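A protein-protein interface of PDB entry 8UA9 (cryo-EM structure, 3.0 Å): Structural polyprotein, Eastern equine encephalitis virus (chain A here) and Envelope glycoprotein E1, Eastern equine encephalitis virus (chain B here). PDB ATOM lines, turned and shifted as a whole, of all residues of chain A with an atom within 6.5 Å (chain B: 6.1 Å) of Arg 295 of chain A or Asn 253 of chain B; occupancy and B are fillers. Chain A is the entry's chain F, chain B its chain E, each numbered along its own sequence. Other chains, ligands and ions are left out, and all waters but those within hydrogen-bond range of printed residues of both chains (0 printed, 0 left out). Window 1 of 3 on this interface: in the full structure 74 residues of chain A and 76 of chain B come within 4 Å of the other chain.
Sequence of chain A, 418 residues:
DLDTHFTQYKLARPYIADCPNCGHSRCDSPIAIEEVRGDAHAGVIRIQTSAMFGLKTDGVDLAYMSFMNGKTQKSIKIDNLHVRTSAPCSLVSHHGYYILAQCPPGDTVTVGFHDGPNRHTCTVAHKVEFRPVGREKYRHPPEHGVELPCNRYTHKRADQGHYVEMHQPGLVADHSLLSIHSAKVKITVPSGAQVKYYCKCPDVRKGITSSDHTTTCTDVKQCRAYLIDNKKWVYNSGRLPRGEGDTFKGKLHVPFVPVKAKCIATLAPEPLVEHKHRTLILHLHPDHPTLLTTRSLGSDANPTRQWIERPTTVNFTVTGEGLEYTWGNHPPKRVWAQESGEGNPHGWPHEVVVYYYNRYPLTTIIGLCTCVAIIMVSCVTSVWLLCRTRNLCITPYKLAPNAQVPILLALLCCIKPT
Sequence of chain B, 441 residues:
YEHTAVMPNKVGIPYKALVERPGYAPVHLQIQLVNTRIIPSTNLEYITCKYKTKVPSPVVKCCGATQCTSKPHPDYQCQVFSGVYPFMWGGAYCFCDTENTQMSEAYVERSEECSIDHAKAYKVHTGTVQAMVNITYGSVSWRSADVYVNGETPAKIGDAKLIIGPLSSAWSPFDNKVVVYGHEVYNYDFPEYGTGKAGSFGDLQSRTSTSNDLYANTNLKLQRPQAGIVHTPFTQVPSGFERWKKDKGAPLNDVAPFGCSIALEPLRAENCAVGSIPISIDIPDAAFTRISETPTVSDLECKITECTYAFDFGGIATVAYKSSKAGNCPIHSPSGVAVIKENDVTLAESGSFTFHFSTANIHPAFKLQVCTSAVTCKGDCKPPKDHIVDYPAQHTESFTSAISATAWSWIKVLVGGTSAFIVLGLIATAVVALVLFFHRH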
ATOM      1  N   THR A 293      23.271 -19.771 -28.879  1.00  0.00           N
ATOM      2  CA  THR A 293      23.137 -21.210 -28.947  1.00  0.00           C
ATOM      3  C   THR A 293      21.833 -21.589 -28.294  1.00  0.00           C
ATOM      4  O   THR A 293      21.466 -21.028 -27.267  1.00  0.00           O
ATOM      5  CB  THR A 293      24.273 -21.937 -28.261  1.00  0.00           C
ATOM      6  OG1 THR A 293      24.431 -21.430 -26.934  1.00  0.00           O
ATOM      7  CG2 THR A 293      25.552 -21.757 -29.023  1.00  0.00           C
ATOM      8  N   THR A 294      21.117 -22.504 -28.920  1.00  0.00           N
ATOM      9  CA  THR A 294      19.864 -23.003 -28.401  1.00  0.00           C
ATOM     10  C   THR A 294      19.863 -24.509 -28.485  1.00  0.00           C
ATOM     11  O   THR A 294      20.502 -25.097 -29.356  1.00  0.00           O
ATOM     12  CB  THR A 294      18.668 -22.464 -29.157  1.00  0.00           C
ATOM     13  OG1 THR A 294      18.766 -22.841 -30.531  1.00  0.00           O
ATOM     14  CG2 THR A 294      18.612 -20.960 -29.050  1.00  0.00           C
ATOM     15  N   ARG A 295      19.133 -25.126 -27.569  1.00  0.00           N
ATOM     16  CA  ARG A 295      18.903 -26.554 -27.637  1.00  0.00           C
ATOM     17  C   ARG A 295      17.595 -26.893 -26.960  1.00  0.00           C
ATOM     18  O   ARG A 295      17.212 -26.268 -25.976  1.00  0.00           O
ATOM     19  CB  ARG A 295      20.026 -27.340 -26.986  1.00  0.00           C
ATOM     20  CG  ARG A 295      20.353 -26.924 -25.607  1.00  0.00           C
ATOM     21  CD  ARG A 295      20.708 -28.091 -24.780  1.00  0.00           C
ATOM     22  NE  ARG A 295      21.466 -27.690 -23.612  1.00  0.00           N
ATOM     23  CZ  ARG A 295      21.831 -28.506 -22.640  1.00  0.00           C
ATOM     24  NH1 ARG A 295      21.626 -29.806 -22.716  1.00  0.00           N
ATOM     25  NH2 ARG A 295      22.413 -28.005 -21.563  1.00  0.00           N
ATOM     26  N   SER A 296      16.928 -27.910 -27.478  1.00  0.00           N
ATOM     27  CA  SER A 296      15.698 -28.396 -26.890  1.00  0.00           C
ATOM     28  C   SER A 296      16.042 -29.411 -25.828  1.00  0.00           C
ATOM     29  O   SER A 296      16.988 -30.184 -25.976  1.00  0.00           O
ATOM     30  CB  SER A 296      14.802 -29.024 -27.943  1.00  0.00           C
ATOM     31  OG  SER A 296      14.913 -30.430 -27.913  1.00  0.00           O
ATOM     32  N   LEU A 297      15.283 -29.403 -24.750  1.00  0.00           N
ATOM     33  CA  LEU A 297      15.576 -30.229 -23.600  1.00  0.00           C
ATOM     34  C   LEU A 297      14.975 -31.619 -23.698  1.00  0.00           C
ATOM     35  O   LEU A 297      14.815 -32.278 -22.670  1.00  0.00           O
ATOM     36  CB  LEU A 297      15.115 -29.532 -22.332  1.00  0.00           C
ATOM     37  CG  LEU A 297      15.696 -28.146 -22.103  1.00  0.00           C
ATOM     38  CD1 LEU A 297      15.045 -27.562 -20.909  1.00  0.00           C
ATOM     39  CD2 LEU A 297      17.181 -28.170 -21.925  1.00  0.00           C
ATOM     40  N   GLY A 298      14.617 -32.071 -24.892  1.00  0.00           N
ATOM     41  CA  GLY A 298      14.029 -33.368 -25.100  1.00  0.00           C
ATOM     42  C   GLY A 298      15.006 -34.373 -25.660  1.00  0.00           C
ATOM     43  O   GLY A 298      16.226 -34.229 -25.547  1.00  0.00           O
ATOM     44  N   ASP A 300      15.686 -35.203 -28.785  1.00  0.00           N
ATOM     45  CA  ASP A 300      16.484 -34.619 -29.848  1.00  0.00           C
ATOM     46  C   ASP A 300      16.790 -33.210 -29.379  1.00  0.00           C
ATOM     47  O   ASP A 300      15.875 -32.426 -29.124  1.00  0.00           O
ATOM     48  CB  ASP A 300      15.711 -34.663 -31.173  1.00  0.00           C
ATOM     49  CG  ASP A 300      16.309 -33.787 -32.301  1.00  0.00           C
ATOM     50  OD1 ASP A 300      16.830 -32.669 -32.104  1.00  0.00           O
ATOM     51  OD2 ASP A 300      16.239 -34.258 -33.456  1.00  0.00           O
ATOM     52  N   ALA A 301      18.072 -32.903 -29.254  1.00  0.00           N
ATOM     53  CA  ALA A 301      18.473 -31.571 -28.850  1.00  0.00           C
ATOM     54  C   ALA A 301      18.046 -30.545 -29.874  1.00  0.00           C
ATOM     55  O   ALA A 301      17.548 -29.472 -29.522  1.00  0.00           O
ATOM     56  CB  ALA A 301      19.973 -31.529 -28.647  1.00  0.00           C
ATOM     57  N   ASN A 302      18.188 -30.876 -31.144  1.00  0.00           N
ATOM     58  CA  ASN A 302      18.076 -29.919 -32.233  1.00  0.00           C
ATOM     59  C   ASN A 302      18.926 -28.678 -31.944  1.00  0.00           C
ATOM     60  O   ASN A 302      18.419 -27.561 -31.906  1.00  0.00           O
ATOM     61  CB  ASN A 302      16.619 -29.547 -32.474  1.00  0.00           C
ATOM     62  CG  ASN A 302      16.311 -29.372 -33.935  1.00  0.00           C
ATOM     63  OD1 ASN A 302      16.932 -28.559 -34.615  1.00  0.00           O
ATOM     64  ND2 ASN A 302      15.354 -30.142 -34.436  1.00  0.00           N
ATOM     65  N   PRO A 303      20.226 -28.857 -31.728  1.00  0.00           N
ATOM     66  CA  PRO A 303      21.059 -27.715 -31.374  1.00  0.00           C
ATOM     67  C   PRO A 303      21.169 -26.746 -32.527  1.00  0.00           C
ATOM     68  O   PRO A 303      21.197 -27.143 -33.689  1.00  0.00           O
ATOM     69  CB  PRO A 303      22.406 -28.348 -31.039  1.00  0.00           C
ATOM     70  CG  PRO A 303      22.404 -29.656 -31.673  1.00  0.00           C
ATOM     71  CD  PRO A 303      21.034 -30.011 -32.124  1.00  0.00           C
ATOM     72  N   THR A 304      21.189 -25.462 -32.195  1.00  0.00           N
ATOM     73  CA  THR A 304      21.420 -24.405 -33.166  1.00  0.00           C
ATOM     74  C   THR A 304      22.483 -23.485 -32.609  1.00  0.00           C
ATOM     75  O   THR A 304      22.393 -23.083 -31.452  1.00  0.00           O
ATOM     76  CB  THR A 304      20.159 -23.603 -33.460  1.00  0.00           C
ATOM     77  OG1 THR A 304      20.074 -22.506 -32.550  1.00  0.00           O
ATOM     78  CG2 THR A 304      18.916 -24.461 -33.321  1.00  0.00           C
ATOM     79  N   GLY A 322      10.768 -28.133 -23.532  1.00  0.00           N
ATOM     80  CA  GLY A 322      11.579 -27.003 -23.140  1.00  0.00           C
ATOM     81  C   GLY A 322      12.616 -26.646 -24.182  1.00  0.00           C
ATOM     82  O   GLY A 322      12.916 -27.403 -25.099  1.00  0.00           O
ATOM     83  N   LEU A 323      13.155 -25.452 -24.004  1.00  0.00           N
ATOM     84  CA  LEU A 323      14.253 -24.930 -24.791  1.00  0.00           C
ATOM     85  C   LEU A 323      15.187 -24.221 -23.836  1.00  0.00           C
ATOM     86  O   LEU A 323      14.772 -23.778 -22.770  1.00  0.00           O
ATOM     87  CB  LEU A 323      13.775 -23.959 -25.857  1.00  0.00           C
ATOM     88  CG  LEU A 323      14.726 -23.669 -26.998  1.00  0.00           C
ATOM     89  CD1 LEU A 323      14.552 -24.684 -28.086  1.00  0.00           C
ATOM     90  CD2 LEU A 323      14.509 -22.299 -27.527  1.00  0.00           C
ATOM     91  N   GLU A 324      16.445 -24.127 -24.221  1.00  0.00           N
ATOM     92  CA  GLU A 324      17.488 -23.476 -23.443  1.00  0.00           C
ATOM     93  C   GLU A 324      18.302 -22.654 -24.409  1.00  0.00           C
ATOM     94  O   GLU A 324      18.833 -23.211 -25.367  1.00  0.00           O
ATOM     95  CB  GLU A 324      18.380 -24.487 -22.740  1.00  0.00           C
ATOM     96  CG  GLU A 324      19.417 -23.900 -21.816  1.00  0.00           C
ATOM     97  CD  GLU A 324      20.570 -24.832 -21.569  1.00  0.00           C
ATOM     98  OE1 GLU A 324      20.954 -24.989 -20.395  1.00  0.00           O
ATOM     99  OE2 GLU A 324      21.106 -25.405 -22.539  1.00  0.00           O
ATOM    100  N   TYR A 325      18.411 -21.355 -24.162  1.00  0.00           N
ATOM    101  CA  TYR A 325      19.169 -20.469 -25.027  1.00  0.00           C
ATOM    102  C   TYR A 325      20.210 -19.731 -24.217  1.00  0.00           C
ATOM    103  O   TYR A 325      19.929 -19.248 -23.118  1.00  0.00           O
ATOM    104  CB  TYR A 325      18.276 -19.471 -25.756  1.00  0.00           C
ATOM    105  CG  TYR A 325      17.586 -18.411 -24.939  1.00  0.00           C
ATOM    106  CD1 TYR A 325      16.331 -18.624 -24.433  1.00  0.00           C
ATOM    107  CD2 TYR A 325      18.154 -17.176 -24.745  1.00  0.00           C
ATOM    108  CE1 TYR A 325      15.689 -17.666 -23.721  1.00  0.00           C
ATOM    109  CE2 TYR A 325      17.514 -16.218 -24.032  1.00  0.00           C
ATOM    110  CZ  TYR A 325      16.282 -16.468 -23.526  1.00  0.00           C
ATOM    111  OH  TYR A 325      15.630 -15.510 -22.808  1.00  0.00           O
ATOM    112  N   ARG A 334      16.272 -21.074 -19.627  1.00  0.00           N
ATOM    113  CA  ARG A 334      15.380 -22.127 -20.081  1.00  0.00           C
ATOM    114  C   ARG A 334      13.952 -21.632 -20.077  1.00  0.00           C
ATOM    115  O   ARG A 334      13.505 -20.995 -19.124  1.00  0.00           O
ATOM    116  CB  ARG A 334      15.438 -23.370 -19.220  1.00  0.00           C
ATOM    117  CG  ARG A 334      16.787 -23.754 -18.800  1.00  0.00           C
ATOM    118  CD  ARG A 334      16.837 -25.120 -18.222  1.00  0.00           C
ATOM    119  NE  ARG A 334      18.147 -25.715 -18.424  1.00  0.00           N
ATOM    120  CZ  ARG A 334      18.410 -27.008 -18.341  1.00  0.00           C
ATOM    121  NH1 ARG A 334      17.473 -27.890 -18.043  1.00  0.00           N
ATOM    122  NH2 ARG A 334      19.644 -27.432 -18.569  1.00  0.00           N
ATOM    123  N   HIS B 183      36.630 -25.999 -19.549  1.00  0.00           N
ATOM    124  CA  HIS B 183      35.350 -26.409 -19.009  1.00  0.00           C
ATOM    125  C   HIS B 183      34.443 -27.019 -20.059  1.00  0.00           C
ATOM    126  O   HIS B 183      33.302 -27.349 -19.737  1.00  0.00           O
ATOM    127  CB  HIS B 183      34.648 -25.219 -18.357  1.00  0.00           C
ATOM    128  CG  HIS B 183      34.117 -24.221 -19.337  1.00  0.00           C
ATOM    129  ND1 HIS B 183      34.934 -23.457 -20.139  1.00  0.00           N
ATOM    130  CD2 HIS B 183      32.850 -23.860 -19.640  1.00  0.00           C
ATOM    131  CE1 HIS B 183      34.194 -22.671 -20.898  1.00  0.00           C
ATOM    132  NE2 HIS B 183      32.924 -22.896 -20.615  1.00  0.00           N
ATOM    133  N   GLU B 184      34.904 -27.171 -21.292  1.00  0.00           N
ATOM    134  CA  GLU B 184      34.126 -27.788 -22.350  1.00  0.00           C
ATOM    135  C   GLU B 184      34.482 -29.258 -22.529  1.00  0.00           C
ATOM    136  O   GLU B 184      35.616 -29.672 -22.293  1.00  0.00           O
ATOM    137  CB  GLU B 184      34.354 -27.026 -23.646  1.00  0.00           C
ATOM    138  CG  GLU B 184      33.958 -25.567 -23.558  1.00  0.00           C
ATOM    139  CD  GLU B 184      34.300 -24.788 -24.804  1.00  0.00           C
ATOM    140  OE1 GLU B 184      34.923 -25.366 -25.714  1.00  0.00           O
ATOM    141  OE2 GLU B 184      33.944 -23.591 -24.876  1.00  0.00           O
ATOM    142  N   VAL B 185      33.499 -30.037 -22.975  1.00  0.00           N
ATOM    143  CA  VAL B 185      33.661 -31.447 -23.305  1.00  0.00           C
ATOM    144  C   VAL B 185      33.140 -31.691 -24.711  1.00  0.00           C
ATOM    145  O   VAL B 185      32.056 -31.223 -25.059  1.00  0.00           O
ATOM    146  CB  VAL B 185      32.940 -32.340 -22.289  1.00  0.00           C
ATOM    147  CG1 VAL B 185      33.149 -33.783 -22.618  1.00  0.00           C
ATOM    148  CG2 VAL B 185      33.428 -32.028 -20.913  1.00  0.00           C
ATOM    149  N   ALA B 250      30.982 -27.403 -31.510  1.00  0.00           N
ATOM    150  CA  ALA B 250      30.038 -27.124 -30.447  1.00  0.00           C
ATOM    151  C   ALA B 250      30.265 -28.115 -29.322  1.00  0.00           C
ATOM    152  O   ALA B 250      30.286 -29.318 -29.588  1.00  0.00           O
ATOM    153  CB  ALA B 250      28.609 -27.217 -30.966  1.00  0.00           C
ATOM    154  N   PRO B 251      30.419 -27.703 -28.072  1.00  0.00           N
ATOM    155  CA  PRO B 251      30.672 -28.687 -27.033  1.00  0.00           C
ATOM    156  C   PRO B 251      29.433 -29.510 -26.756  1.00  0.00           C
ATOM    157  O   PRO B 251      28.334 -29.229 -27.230  1.00  0.00           O
ATOM    158  CB  PRO B 251      31.069 -27.843 -25.830  1.00  0.00           C
ATOM    159  CG  PRO B 251      30.589 -26.527 -26.089  1.00  0.00           C
ATOM    160  CD  PRO B 251      30.112 -26.402 -27.482  1.00  0.00           C
ATOM    161  N   LEU B 252      29.628 -30.552 -25.962  1.00  0.00           N
ATOM    162  CA  LEU B 252      28.519 -31.345 -25.473  1.00  0.00           C
ATOM    163  C   LEU B 252      27.721 -30.624 -24.406  1.00  0.00           C
ATOM    164  O   LEU B 252      26.626 -31.072 -24.072  1.00  0.00           O
ATOM    165  CB  LEU B 252      29.062 -32.655 -24.939  1.00  0.00           C
ATOM    166  CG  LEU B 252      28.091 -33.782 -24.708  1.00  0.00           C
ATOM    167  CD1 LEU B 252      27.636 -34.368 -26.017  1.00  0.00           C
ATOM    168  CD2 LEU B 252      28.756 -34.811 -23.863  1.00  0.00           C
ATOM    169  N   ASN B 253      28.216 -29.510 -23.883  1.00  0.00           N
ATOM    170  CA  ASN B 253      27.452 -28.742 -22.917  1.00  0.00           C
ATOM    171  C   ASN B 253      26.247 -28.091 -23.559  1.00  0.00           C
ATOM    172  O   ASN B 253      25.291 -27.754 -22.858  1.00  0.00           O
ATOM    173  CB  ASN B 253      28.329 -27.689 -22.259  1.00  0.00           C
ATOM    174  CG  ASN B 253      29.625 -28.252 -21.770  1.00  0.00           C
ATOM    175  OD1 ASN B 253      29.913 -29.423 -21.972  1.00  0.00           O
ATOM    176  ND2 ASN B 253      30.419 -27.429 -21.124  1.00  0.00           N
ATOM    177  N   ASP B 254      26.282 -27.896 -24.870  1.00  0.00           N
ATOM    178  CA  ASP B 254      25.208 -27.318 -25.653  1.00  0.00           C
ATOM    179  C   ASP B 254      24.449 -28.359 -26.457  1.00  0.00           C
ATOM    180  O   ASP B 254      23.225 -28.302 -26.533  1.00  0.00           O
ATOM    181  CB  ASP B 254      25.774 -26.265 -26.589  1.00  0.00           C
ATOM    182  CG  ASP B 254      26.716 -25.328 -25.890  1.00  0.00           C
ATOM    183  OD1 ASP B 254      26.746 -25.349 -24.645  1.00  0.00           O
ATOM    184  OD2 ASP B 254      27.429 -24.571 -26.578  1.00  0.00           O
ATOM    185  N   VAL B 255      25.154 -29.273 -27.110  1.00  0.00           N
ATOM    186  CA  VAL B 255      24.511 -30.309 -27.905  1.00  0.00           C
ATOM    187  C   VAL B 255      23.649 -31.227 -27.043  1.00  0.00           C
ATOM    188  O   VAL B 255      22.611 -31.710 -27.497  1.00  0.00           O
ATOM    189  CB  VAL B 255      25.580 -31.094 -28.678  1.00  0.00           C
ATOM    190  CG1 VAL B 255      24.975 -32.330 -29.340  1.00  0.00           C
ATOM    191  CG2 VAL B 255      26.235 -30.196 -29.697  1.00  0.00           C
ATOM    192  N   ALA B 256      24.080 -31.525 -25.833  1.00  0.00           N
ATOM    193  CA  ALA B 256      23.577 -32.605 -24.979  1.00  0.00           C
ATOM    194  C   ALA B 256      22.064 -32.810 -24.903  1.00  0.00           C
ATOM    195  O   ALA B 256      21.352 -31.891 -24.493  1.00  0.00           O
ATOM    196  CB  ALA B 256      24.058 -32.377 -23.557  1.00  0.00           C
ATOM    197  N   PRO B 257      21.526 -33.979 -25.256  1.00  0.00           N
ATOM    198  CA  PRO B 257      20.094 -34.209 -25.072  1.00  0.00           C
ATOM    199  C   PRO B 257      19.684 -34.261 -23.615  1.00  0.00           C
ATOM    200  O   PRO B 257      20.491 -34.458 -22.710  1.00  0.00           O
ATOM    201  CB  PRO B 257      19.846 -35.556 -25.742  1.00  0.00           C
ATOM    202  CG  PRO B 257      20.984 -35.851 -26.519  1.00  0.00           C
ATOM    203  CD  PRO B 257      22.109 -34.969 -26.171  1.00  0.00           C
ATOM    204  N   PHE B 258      18.384 -34.072 -23.405  1.00  0.00           N
ATOM    205  CA  PHE B 258      17.702 -34.147 -22.118  1.00  0.00           C
ATOM    206  C   PHE B 258      18.081 -33.048 -21.140  1.00  0.00           C
ATOM    207  O   PHE B 258      17.679 -33.100 -19.988  1.00  0.00           O
ATOM    208  CB  PHE B 258      17.905 -35.509 -21.469  1.00  0.00           C
ATOM    209  CG  PHE B 258      17.310 -36.616 -22.251  1.00  0.00           C
ATOM    210  CD1 PHE B 258      15.954 -36.746 -22.352  1.00  0.00           C
ATOM    211  CD2 PHE B 258      18.100 -37.509 -22.917  1.00  0.00           C
ATOM    212  CE1 PHE B 258      15.409 -37.740 -23.078  1.00  0.00           C
ATOM    213  CE2 PHE B 258      17.545 -38.509 -23.645  1.00  0.00           C
ATOM    214  CZ  PHE B 258      16.206 -38.621 -23.725  1.00  0.00           C
ATOM    215  N   GLY B 259      18.819 -32.043 -21.572  1.00  0.00           N
ATOM    216  CA  GLY B 259      19.182 -30.958 -20.692  1.00  0.00           C
ATOM    217  C   GLY B 259      20.221 -31.382 -19.696  1.00  0.00           C
ATOM    218  O   GLY B 259      20.186 -30.951 -18.541  1.00  0.00           O
ATOM    219  N   CYS B 260      21.162 -32.199 -20.132  1.00  0.00           N
ATOM    220  CA  CYS B 260      22.315 -32.555 -19.333  1.00  0.00           C
ATOM    221  C   CYS B 260      23.256 -31.376 -19.211  1.00  0.00           C
ATOM    222  O   CYS B 260      23.586 -30.733 -20.210  1.00  0.00           O
ATOM    223  CB  CYS B 260      23.024 -33.744 -19.950  1.00  0.00           C
ATOM    224  SG  CYS B 260      22.017 -35.197 -19.952  1.00  0.00           S
ATOM    225  N   SER B 261      23.680 -31.086 -17.998  1.00  0.00           N
ATOM    226  CA  SER B 261      24.669 -30.057 -17.732  1.00  0.00           C
ATOM    227  C   SER B 261      25.985 -30.745 -17.419  1.00  0.00           C
ATOM    228  O   SER B 261      26.053 -31.549 -16.492  1.00  0.00           O
ATOM    229  CB  SER B 261      24.235 -29.186 -16.561  1.00  0.00           C
ATOM    230  OG  SER B 261      23.146 -28.362 -16.918  1.00  0.00           O
ATOM    231  N   ILE B 262      27.022 -30.458 -18.192  1.00  0.00           N
ATOM    232  CA  ILE B 262      28.279 -31.187 -18.085  1.00  0.00           C
ATOM    233  C   ILE B 262      29.180 -30.434 -17.124  1.00  0.00           C
ATOM    234  O   ILE B 262      29.486 -29.261 -17.348  1.00  0.00           O
ATOM    235  CB  ILE B 262      28.941 -31.344 -19.462  1.00  0.00           C
ATOM    236  CG1 ILE B 262      28.489 -32.616 -20.159  1.00  0.00           C
ATOM    237  CG2 ILE B 262      30.476 -31.419 -19.393  1.00  0.00           C
ATOM    238  CD1 ILE B 262      27.029 -32.887 -20.092  1.00  0.00           C
ATOM    239  N   LEU B 264      32.968 -30.796 -14.739  1.00  0.00           N
ATOM    240  CA  LEU B 264      34.298 -31.272 -15.094  1.00  0.00           C
ATOM    241  C   LEU B 264      35.295 -31.490 -13.967  1.00  0.00           C
ATOM    242  O   LEU B 264      36.434 -31.868 -14.260  1.00  0.00           O
ATOM    243  CB  LEU B 264      34.920 -30.323 -16.117  1.00  0.00           C
ATOM    244  CG  LEU B 264      34.827 -30.920 -17.507  1.00  0.00           C
ATOM    245  CD1 LEU B 264      35.075 -29.851 -18.522  1.00  0.00           C
ATOM    246  CD2 LEU B 264      35.792 -32.069 -17.686  1.00  0.00           C
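The backbone carbonyl oxygen of Asn 253 of chain B sits at hydrogen-bond distance from the guanidinium group of Arg 295 of chain A, at 3.2 Å.
The guanidinium group (NH2) of Arg 295 of chain A sits at hydrogen-bond distance from the backbone carbonyl oxygen (O) of Cys 260 of chain B (3.3 Å).
The backbone carbonyl oxygen of Ala 256 of chain B sits at hydrogen-bond distance from the guanidinium group of Arg 295 of chain A (2.8 Å).
The backbone carbonyl oxygen of Asp 254 of chain B sits close to the guanidinium group of Arg 295 of chain A, 3.5 Å away.
N of Phe 258 of chain B lies within hydrogen-bond range of O of Gly 298 of chain A (3.0 Å).
The backbone NH (N) of Leu 297 of chain A is in hydrogen-bond range of the backbone carbonyl oxygen (O) of Gly 322 of chain A (3.1 Å).
The guanidinium group of Arg 295 of chain A is in salt-bridge range of the side-chain carboxylate of Glu 324 of chain A (2.5 Å).
The side-chain amide nitrogen (ND2) of Asn 253 of chain B lies within hydrogen-bond range of the backbone carbonyl oxygen (O) of His 183 of chain B (3.2 Å).
The guanidinium group (NH2) of Arg 334 of chain A lies within salt-bridge range of the side-chain carboxylate (OE1) of Glu 324 of chain A, at 3.3 Å.
The backbone NH (N) of Ser 296 of chain A lies within hydrogen-bond range of the backbone carbonyl oxygen (O) of Ala 301 of chain A (2.6 Å).
The side-chain hydroxyl (OG) of Ser 296 of chain A sits close to the backbone NH (N) of Gly 298 of chain A.
CA of Gly 259 of chain B touches NH1 of Arg 295 of chain A, at 3.4 Å.
Leu 297 of chain A touches Phe 258 of chain B (O to CA, 3.5 Å).
CA of Gly 259 of chain B touches CD2 of Leu 297 of chain A (3.6 Å).
O of Gly 298 of chain A touches CB of Pro 257 of chain B, 3.9 Å away.
Ala 301 of chain A touches Val 255 of chain B (CB to O, 2.9 Å).
Gly 259 of chain B touches Arg 334 of chain A.
Ser 261 of chain B touches Arg 334 of chain A.
Arg 295 of chain A touches just these residues of chain B: Asn 253, Asp 254, Ala 256, Gly 259 and Cys 260.
Of the printed residues of chain B, Leu 297 of chain A touches Phe 258 (3.5 Å) and Gly 259 (3.6 Å).
Asp 300 of chain A touches none of the printed residues of chain B.
Of the printed residues of chain B, Ala 301 of chain A touches Val 255.
Gly 322 of chain A touches none of the printed residues of chain B.
Printed residues of chain B within 4 Å of Arg 334 of chain A: Gly 259 and Ser 261.
Asn 253 of chain B touches one residue of chain A.
Of the printed residues of chain A, Val 255 of chain B touches Ala 301.
Of the printed residues of chain A, Phe 258 of chain B touches Leu 297 (3.5 Å) and Gly 298 (3.0 Å).
Of the 16 printed residues of chain A, 5 touch a printed residue of chain B.
Among the printed residues, no Asp or Glu carboxylate lies within 4 Å of a Lys or Arg side-chain nitrogen of the other chain.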
